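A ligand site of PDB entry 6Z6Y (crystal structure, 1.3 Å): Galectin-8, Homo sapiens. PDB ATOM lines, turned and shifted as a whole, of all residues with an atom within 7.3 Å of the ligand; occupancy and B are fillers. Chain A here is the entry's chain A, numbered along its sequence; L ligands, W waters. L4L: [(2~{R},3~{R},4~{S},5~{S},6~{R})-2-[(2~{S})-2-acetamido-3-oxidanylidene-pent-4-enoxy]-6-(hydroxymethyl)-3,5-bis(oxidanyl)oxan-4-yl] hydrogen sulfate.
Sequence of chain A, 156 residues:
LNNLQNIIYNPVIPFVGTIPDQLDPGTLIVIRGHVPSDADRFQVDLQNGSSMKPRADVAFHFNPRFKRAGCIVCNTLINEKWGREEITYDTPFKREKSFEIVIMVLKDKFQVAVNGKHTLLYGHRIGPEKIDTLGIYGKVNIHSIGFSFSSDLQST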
ATOM      1  N   ARG A  41       4.316  10.209  -9.702  1.00  0.00           N
ATOM      2  CA  ARG A  41       4.355   8.939 -10.413  1.00  0.00           C
ATOM      3  C   ARG A  41       5.596   8.919 -11.306  1.00  0.00           C
ATOM      4  O   ARG A  41       6.182   9.958 -11.605  1.00  0.00           O
ATOM      5  CB  ARG A  41       3.104   8.744 -11.264  1.00  0.00           C
ATOM      6  CG  ARG A  41       2.828   9.858 -12.267  1.00  0.00           C
ATOM      7  CD  ARG A  41       1.652   9.500 -13.162  1.00  0.00           C
ATOM      8  NE  ARG A  41       2.082   8.704 -14.312  1.00  0.00           N
ATOM      9  CZ  ARG A  41       1.255   8.072 -15.138  1.00  0.00           C
ATOM     10  NH1 ARG A  41      -0.047   8.045 -14.914  1.00  0.00           N
ATOM     11  NH2 ARG A  41       1.746   7.471 -16.211  1.00  0.00           N
ATOM     12  N   GLN A  43       7.212   5.984 -14.602  1.00  0.00           N
ATOM     13  CA  GLN A  43       6.928   4.750 -15.312  1.00  0.00           C
ATOM     14  C   GLN A  43       8.151   4.236 -16.048  1.00  0.00           C
ATOM     15  O   GLN A  43       9.003   5.009 -16.490  1.00  0.00           O
ATOM     16  CB  GLN A  43       5.777   4.950 -16.305  1.00  0.00           C
ATOM     17  CG  GLN A  43       6.152   5.838 -17.487  1.00  0.00           C
ATOM     18  CD  GLN A  43       4.955   6.591 -18.006  1.00  0.00           C
ATOM     19  OE1 GLN A  43       4.379   7.429 -17.312  1.00  0.00           O
ATOM     20  NE2 GLN A  43       4.565   6.304 -19.236  1.00  0.00           N
ATOM     21  N   ASP A  45       8.556   1.892 -19.394  1.00  0.00           N
ATOM     22  CA  ASP A  45       7.786   1.434 -20.535  1.00  0.00           C
ATOM     23  C   ASP A  45       8.689   0.606 -21.446  1.00  0.00           C
ATOM     24  O   ASP A  45       9.741   1.086 -21.879  1.00  0.00           O
ATOM     25  CB  ASP A  45       7.210   2.609 -21.345  1.00  0.00           C
ATOM     26  CG  ASP A  45       6.144   3.368 -20.593  1.00  0.00           C
ATOM     27  OD1 ASP A  45       5.510   2.806 -19.677  1.00  0.00           O
ATOM     28  OD2 ASP A  45       5.851   4.528 -20.980  1.00  0.00           O
ATOM     29  N   ARG A  55       2.182   7.818 -31.109  1.00  0.00           N
ATOM     30  CA  ARG A  55       2.946   7.325 -29.980  1.00  0.00           C
ATOM     31  C   ARG A  55       3.197   5.822 -30.110  1.00  0.00           C
ATOM     32  O   ARG A  55       2.288   5.044 -30.383  1.00  0.00           O
ATOM     33  CB  ARG A  55       2.169   7.630 -28.709  1.00  0.00           C
ATOM     34  CG  ARG A  55       2.879   7.163 -27.480  1.00  0.00           C
ATOM     35  CD  ARG A  55       2.127   7.523 -26.233  1.00  0.00           C
ATOM     36  NE  ARG A  55       2.761   6.957 -25.045  1.00  0.00           N
ATOM     37  CZ  ARG A  55       2.218   7.052 -23.833  1.00  0.00           C
ATOM     38  NH1 ARG A  55       1.061   7.651 -23.643  1.00  0.00           N
ATOM     39  NH2 ARG A  55       2.858   6.514 -22.800  1.00  0.00           N
ATOM     40  N   VAL A  58       3.203   0.414 -26.356  1.00  0.00           N
ATOM     41  CA  VAL A  58       3.883   0.045 -25.125  1.00  0.00           C
ATOM     42  C   VAL A  58       3.417  -1.369 -24.757  1.00  0.00           C
ATOM     43  O   VAL A  58       2.265  -1.565 -24.375  1.00  0.00           O
ATOM     44  CB  VAL A  58       3.599   1.030 -23.974  1.00  0.00           C
ATOM     45  CG1 VAL A  58       4.325   0.589 -22.689  1.00  0.00           C
ATOM     46  CG2 VAL A  58       4.015   2.451 -24.343  1.00  0.00           C
ATOM     47  N   HIS A  61       3.770  -1.317 -19.627  1.00  0.00           N
ATOM     48  CA  HIS A  61       3.814  -0.065 -18.889  1.00  0.00           C
ATOM     49  C   HIS A  61       3.779  -0.427 -17.423  1.00  0.00           C
ATOM     50  O   HIS A  61       2.845  -1.111 -16.981  1.00  0.00           O
ATOM     51  CB  HIS A  61       2.585   0.723 -19.316  1.00  0.00           C
ATOM     52  CG  HIS A  61       2.272   1.958 -18.527  1.00  0.00           C
ATOM     53  ND1 HIS A  61       3.037   3.104 -18.589  1.00  0.00           N
ATOM     54  CD2 HIS A  61       1.179   2.272 -17.793  1.00  0.00           C
ATOM     55  CE1 HIS A  61       2.419   4.071 -17.905  1.00  0.00           C
ATOM     56  NE2 HIS A  61       1.309   3.570 -17.394  1.00  0.00           N
ATOM     57  N   ASN A  63       3.992   1.357 -13.852  1.00  0.00           N
ATOM     58  CA  ASN A  63       3.711   2.740 -13.481  1.00  0.00           C
ATOM     59  C   ASN A  63       3.422   2.884 -11.983  1.00  0.00           C
ATOM     60  O   ASN A  63       2.230   2.887 -11.586  1.00  0.00           O
ATOM     61  CB  ASN A  63       2.569   3.254 -14.351  1.00  0.00           C
ATOM     62  CG  ASN A  63       2.057   4.637 -13.994  1.00  0.00           C
ATOM     63  OD1 ASN A  63       0.881   4.932 -14.183  1.00  0.00           O
ATOM     64  ND2 ASN A  63       2.955   5.523 -13.551  1.00  0.00           N
ATOM     65  N   ARG A  65       2.583   4.821  -8.734  1.00  0.00           N
ATOM     66  CA  ARG A  65       1.873   6.047  -8.410  1.00  0.00           C
ATOM     67  C   ARG A  65       1.888   6.250  -6.901  1.00  0.00           C
ATOM     68  O   ARG A  65       1.703   5.300  -6.138  1.00  0.00           O
ATOM     69  CB  ARG A  65       0.432   5.974  -8.910  1.00  0.00           C
ATOM     70  CG  ARG A  65       0.342   5.840 -10.409  1.00  0.00           C
ATOM     71  CD  ARG A  65      -1.084   5.759 -10.904  1.00  0.00           C
ATOM     72  NE  ARG A  65      -1.111   5.633 -12.354  1.00  0.00           N
ATOM     73  CZ  ARG A  65      -2.218   5.668 -13.073  1.00  0.00           C
ATOM     74  NH1 ARG A  65      -3.399   5.850 -12.517  1.00  0.00           N
ATOM     75  NH2 ARG A  65      -2.143   5.474 -14.384  1.00  0.00           N
ATOM     76  N   ARG A  68      -2.468   9.121  -2.585  1.00  0.00           N
ATOM     77  CA  ARG A  68      -3.393   8.317  -1.794  1.00  0.00           C
ATOM     78  C   ARG A  68      -2.610   7.187  -1.136  1.00  0.00           C
ATOM     79  O   ARG A  68      -1.599   7.471  -0.467  1.00  0.00           O
ATOM     80  CB  ARG A  68      -4.571   7.907  -2.665  1.00  0.00           C
ATOM     81  CG  ARG A  68      -5.365   9.085  -3.173  1.00  0.00           C
ATOM     82  CD  ARG A  68      -6.357   8.701  -4.246  1.00  0.00           C
ATOM     83  NE  ARG A  68      -7.091   9.870  -4.743  1.00  0.00           N
ATOM     84  CZ  ARG A  68      -6.932  10.387  -5.954  1.00  0.00           C
ATOM     85  NH1 ARG A  68      -6.064   9.886  -6.817  1.00  0.00           N
ATOM     86  NH2 ARG A  68      -7.672  11.445  -6.307  1.00  0.00           N
ATOM     87  N   VAL A  73       0.344   0.677 -11.436  1.00  0.00           N
ATOM     88  CA  VAL A  73      -0.548   0.388 -12.548  1.00  0.00           C
ATOM     89  C   VAL A  73       0.290  -0.224 -13.668  1.00  0.00           C
ATOM     90  O   VAL A  73       1.334   0.338 -14.025  1.00  0.00           O
ATOM     91  CB  VAL A  73      -1.239   1.667 -13.029  1.00  0.00           C
ATOM     92  CG1 VAL A  73      -2.033   1.435 -14.299  1.00  0.00           C
ATOM     93  CG2 VAL A  73      -2.099   2.272 -11.938  1.00  0.00           C
ATOM     94  N   CYS A  74      -0.170  -1.344 -14.223  1.00  0.00           N
ATOM     95  CA  CYS A  74       0.440  -1.940 -15.393  1.00  0.00           C
ATOM     96  C   CYS A  74      -0.588  -2.015 -16.506  1.00  0.00           C
ATOM     97  O   CYS A  74      -1.782  -2.234 -16.262  1.00  0.00           O
ATOM     98  CB  CYS A  74       1.009  -3.323 -15.065  1.00  0.00           C
ATOM     99  SG  CYS A  74       2.303  -3.358 -13.901  1.00  0.00           S
ATOM    100  N   ASN A  75      -0.131  -1.829 -17.735  1.00  0.00           N
ATOM    101  CA  ASN A  75      -1.051  -1.792 -18.863  1.00  0.00           C
ATOM    102  C   ASN A  75      -0.232  -1.951 -20.142  1.00  0.00           C
ATOM    103  O   ASN A  75       0.987  -2.018 -20.113  1.00  0.00           O
ATOM    104  CB  ASN A  75      -1.885  -0.499 -18.840  1.00  0.00           C
ATOM    105  CG  ASN A  75      -3.233  -0.638 -19.539  1.00  0.00           C
ATOM    106  OD1 ASN A  75      -3.495  -1.589 -20.277  1.00  0.00           O
ATOM    107  ND2 ASN A  75      -4.124   0.336 -19.297  1.00  0.00           N
ATOM    108  N   THR A  76      -0.959  -1.949 -21.268  1.00  0.00           N
ATOM    109  CA  THR A  76      -0.408  -2.027 -22.619  1.00  0.00           C
ATOM    110  C   THR A  76      -1.118  -0.989 -23.481  1.00  0.00           C
ATOM    111  O   THR A  76      -2.343  -0.806 -23.384  1.00  0.00           O
ATOM    112  CB  THR A  76      -0.673  -3.434 -23.160  1.00  0.00           C
ATOM    113  OG1 THR A  76       0.089  -4.397 -22.412  1.00  0.00           O
ATOM    114  CG2 THR A  76      -0.353  -3.564 -24.627  1.00  0.00           C
ATOM    115  N   LEU A  77      -0.337  -0.263 -24.277  1.00  0.00           N
ATOM    116  CA  LEU A  77      -0.828   0.777 -25.173  1.00  0.00           C
ATOM    117  C   LEU A  77      -0.675   0.257 -26.601  1.00  0.00           C
ATOM    118  O   LEU A  77       0.421  -0.099 -27.028  1.00  0.00           O
ATOM    119  CB  LEU A  77       0.011   2.040 -24.980  1.00  0.00           C
ATOM    120  CG  LEU A  77      -0.406   3.226 -25.875  1.00  0.00           C
ATOM    121  CD1 LEU A  77      -1.607   3.954 -25.282  1.00  0.00           C
ATOM    122  CD2 LEU A  77       0.734   4.212 -26.087  1.00  0.00           C
ATOM    123  N   TRP A  82      -5.073   2.855 -24.460  1.00  0.00           N
ATOM    124  CA  TRP A  82      -4.695   1.983 -23.361  1.00  0.00           C
ATOM    125  C   TRP A  82      -5.709   0.862 -23.214  1.00  0.00           C
ATOM    126  O   TRP A  82      -6.910   1.032 -23.495  1.00  0.00           O
ATOM    127  CB  TRP A  82      -4.652   2.807 -22.078  1.00  0.00           C
ATOM    128  CG  TRP A  82      -3.461   3.684 -21.988  1.00  0.00           C
ATOM    129  CD1 TRP A  82      -3.408   5.049 -22.172  1.00  0.00           C
ATOM    130  CD2 TRP A  82      -2.116   3.271 -21.718  1.00  0.00           C
ATOM    131  NE1 TRP A  82      -2.129   5.481 -22.012  1.00  0.00           N
ATOM    132  CE2 TRP A  82      -1.310   4.417 -21.760  1.00  0.00           C
ATOM    133  CE3 TRP A  82      -1.508   2.040 -21.481  1.00  0.00           C
ATOM    134  CZ2 TRP A  82       0.056   4.368 -21.545  1.00  0.00           C
ATOM    135  CZ3 TRP A  82      -0.139   2.009 -21.266  1.00  0.00           C
ATOM    136  CH2 TRP A  82       0.621   3.167 -21.293  1.00  0.00           C
ATOM    137  N   GLY A  83      -5.230  -0.298 -22.784  1.00  0.00           N
ATOM    138  CA  GLY A  83      -6.062  -1.446 -22.527  1.00  0.00           C
ATOM    139  C   GLY A  83      -6.554  -1.435 -21.095  1.00  0.00           C
ATOM    140  O   GLY A  83      -6.637  -0.398 -20.454  1.00  0.00           O
ATOM    141  N   ARG A  84      -6.889  -2.630 -20.613  1.00  0.00           N
ATOM    142  CA  ARG A  84      -7.380  -2.760 -19.249  1.00  0.00           C
ATOM    143  C   ARG A  84      -6.197  -2.731 -18.263  1.00  0.00           C
ATOM    144  O   ARG A  84      -5.245  -3.504 -18.398  1.00  0.00           O
ATOM    145  CB  ARG A  84      -8.134  -4.071 -19.124  1.00  0.00           C
ATOM    146  CG  ARG A  84      -8.407  -4.531 -17.706  1.00  0.00           C
ATOM    147  CD  ARG A  84      -9.170  -3.491 -16.900  1.00  0.00           C
ATOM    148  NE  ARG A  84     -10.600  -3.767 -16.825  1.00  0.00           N
ATOM    149  CZ  ARG A  84     -11.172  -4.664 -16.030  1.00  0.00           C
ATOM    150  NH1 ARG A  84     -10.460  -5.463 -15.253  1.00  0.00           N
ATOM    151  NH2 ARG A  84     -12.498  -4.763 -16.034  1.00  0.00           N
ATOM    152  N   GLU A  85      -6.268  -1.842 -17.271  1.00  0.00           N
ATOM    153  CA  GLU A  85      -5.232  -1.732 -16.246  1.00  0.00           C
ATOM    154  C   GLU A  85      -5.228  -2.921 -15.295  1.00  0.00           C
ATOM    155  O   GLU A  85      -6.286  -3.435 -14.937  1.00  0.00           O
ATOM    156  CB  GLU A  85      -5.483  -0.471 -15.394  1.00  0.00           C
ATOM    157  CG  GLU A  85      -5.300   0.817 -16.127  1.00  0.00           C
ATOM    158  CD  GLU A  85      -5.523   2.068 -15.273  1.00  0.00           C
ATOM    159  OE1 GLU A  85      -4.958   3.129 -15.616  1.00  0.00           O
ATOM    160  OE2 GLU A  85      -6.264   1.995 -14.278  1.00  0.00           O
ATOM    161  N   GLU A  86      -4.036  -3.330 -14.867  1.00  0.00           N
ATOM    162  CA  GLU A  86      -3.844  -4.273 -13.764  1.00  0.00           C
ATOM    163  C   GLU A  86      -3.166  -3.527 -12.634  1.00  0.00           C
ATOM    164  O   GLU A  86      -2.064  -2.997 -12.809  1.00  0.00           O
ATOM    165  CB  GLU A  86      -3.008  -5.478 -14.198  1.00  0.00           C
ATOM    166  CG  GLU A  86      -3.660  -6.286 -15.302  1.00  0.00           C
ATOM    167  CD  GLU A  86      -2.839  -7.448 -15.765  1.00  0.00           C
ATOM    168  OE1 GLU A  86      -1.929  -7.891 -15.030  1.00  0.00           O
ATOM    169  OE2 GLU A  86      -3.123  -7.932 -16.879  1.00  0.00           O
ATOM    170  N   TYR A 137       9.913   7.649 -17.692  1.00  0.00           N
ATOM    171  CA  TYR A 137       9.302   8.961 -17.666  1.00  0.00           C
ATOM    172  C   TYR A 137       8.804   9.265 -16.264  1.00  0.00           C
ATOM    173  O   TYR A 137       8.575   8.356 -15.465  1.00  0.00           O
ATOM    174  CB  TYR A 137       8.142   9.080 -18.681  1.00  0.00           C
ATOM    175  CG  TYR A 137       8.444   8.491 -20.051  1.00  0.00           C
ATOM    176  CD1 TYR A 137       8.159   7.163 -20.342  1.00  0.00           C
ATOM    177  CD2 TYR A 137       8.956   9.276 -21.075  1.00  0.00           C
ATOM    178  CE1 TYR A 137       8.446   6.616 -21.578  1.00  0.00           C
ATOM    179  CE2 TYR A 137       9.229   8.737 -22.315  1.00  0.00           C
ATOM    180  CZ  TYR A 137       8.966   7.411 -22.570  1.00  0.00           C
ATOM    181  OH  TYR A 137       9.224   6.880 -23.815  1.00  0.00           O
HETATM  182  C01 L4L L   1      -6.257   9.542 -14.057  1.00  0.00           C
HETATM  183  C02 L4L L   1      -6.498   9.087 -15.292  1.00  0.00           C
HETATM  184  C03 L4L L   1      -7.052   7.894 -15.992  1.00  0.00           C
HETATM  185  C04 L4L L   1      -6.987   8.012 -17.520  1.00  0.00           C
HETATM  186  C06 L4L L   1      -7.390  10.137 -18.815  1.00  0.00           C
HETATM  187  C07 L4L L   1      -8.870   9.765 -19.033  1.00  0.00           C
HETATM  188  C09 L4L L   1      -5.907   6.916 -17.786  1.00  0.00           C
HETATM  189  C11 L4L L   1      -3.673   6.925 -18.050  1.00  0.00           C
HETATM  190  C12 L4L L   1      -2.419   7.788 -18.028  1.00  0.00           C
HETATM  191  C14 L4L L   1      -1.343   7.062 -18.756  1.00  0.00           C
HETATM  192  C20 L4L L   1      -1.134   5.669 -18.296  1.00  0.00           C
HETATM  193  C22 L4L L   1      -2.445   4.873 -18.324  1.00  0.00           C
HETATM  194  C23 L4L L   1      -2.304   3.502 -17.790  1.00  0.00           C
HETATM  195  N05 L4L L   1      -6.492   9.253 -18.072  1.00  0.00           N
HETATM  196  O08 L4L L   1      -6.980  11.158 -19.272  1.00  0.00           O
HETATM  197  O10 L4L L   1      -4.665   7.498 -17.333  1.00  0.00           O
HETATM  198  O13 L4L L   1      -2.767   9.021 -18.644  1.00  0.00           O
HETATM  199  O15 L4L L   1      -0.151   7.881 -18.559  1.00  0.00           O
HETATM  200  O17 L4L L   1       0.019   8.156 -21.099  1.00  0.00           O
HETATM  201  O18 L4L L   1       1.781   6.912 -19.980  1.00  0.00           O
HETATM  202  O19 L4L L   1       1.524   9.360 -19.589  1.00  0.00           O
HETATM  203  O21 L4L L   1      -0.494   5.679 -16.976  1.00  0.00           O
HETATM  204  O24 L4L L   1      -3.522   2.774 -17.902  1.00  0.00           O
HETATM  205  O25 L4L L   1      -3.377   5.630 -17.463  1.00  0.00           O
HETATM  206  O26 L4L L   1      -7.262   6.872 -15.457  1.00  0.00           O
HETATM  207  S16 L4L L   1       0.848   8.073 -19.857  1.00  0.00           S
HETATM  208  O   HOH W   1      -3.484   9.179 -21.212  1.00  0.00           O
HETATM  209  O   HOH W   2      -6.050   4.005 -19.135  1.00  0.00           O
HETATM  210  O   HOH W   3      -4.046  10.826 -17.218  1.00  0.00           O
HETATM  211  O   HOH W   4      -5.373   5.552 -14.636  1.00  0.00           O
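Residues that only touch the ligand: Trp 82 (3.4 Å). Hydrophobic or aromatic side chains within 4 Å of the ligand: His 61 and Trp 82. Nine residues have an atom within 4 Å of the ligand: Arg 41, Gln 43, Arg 55, His 61, Asn 63, Arg 65, Asn 75, Trp 82 and Glu 85. The nearest printed residue that does not touch the ligand is Val 73 (4.1 Å).
OE1 of Glu 85 sits at hydrogen-bond distance from O24 of the ligand, at 2.7 Å. An oxygen (O17) of the ligand is in salt-bridge range of the guanidinium group (NH1) of Arg 55 (2.8 Å). A ring nitrogen (NE2) of His 61 is in hydrogen-bond range of an oxygen (O21) of the ligand, 2.8 Å away. An oxygen (O24) of the ligand lies within hydrogen-bond range of the side-chain amide nitrogen (ND2) of Asn 75 (2.9 Å). O18 of the ligand lies within hydrogen-bond range of NE2 of Gln 43, 2.9 Å away. O18 of the ligand is in salt-bridge range of NH2 of Arg 41, 3.8 Å away. An oxygen (O21) of the ligand sits at hydrogen-bond distance from the guanidinium group of Arg 65, at 3.1 Å. OD1 of Asn 63 is in hydrogen-bond range of O21 of the ligand (3.2 Å).
The side-chain carboxylate of Glu 85 lies within salt-bridge range of the guanidinium group of Arg 65. N of His 61 is in hydrogen-bond range of O of Asn 75, 2.9 Å away. A ring nitrogen (ND1) of His 61 lies within hydrogen-bond range of the side-chain carboxylate (OD1) of Asp 45, at 2.7 Å. O of Gly 83 sits at hydrogen-bond distance from ND2 of Asn 75 (2.9 Å). OE1 of Gln 43 sits at hydrogen-bond distance from NH2 of Arg 41 (2.9 Å). NH1 of Arg 41 sits close to OD1 of Asn 63, at 3.3 Å. NE of Arg 65 sits at hydrogen-bond distance from OD1 of Asn 63, at 2.8 Å. The backbone NH (N) of Asn 63 is in hydrogen-bond range of the backbone carbonyl oxygen (O) of Val 73 (2.9 Å).
Water W4 lies within hydrogen-bond range of an oxygen (O26) of the ligand (2.4 Å), the side-chain carboxylate of Glu 85 (2.6 Å) and the guanidinium group of Arg 65 (2.9 Å).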
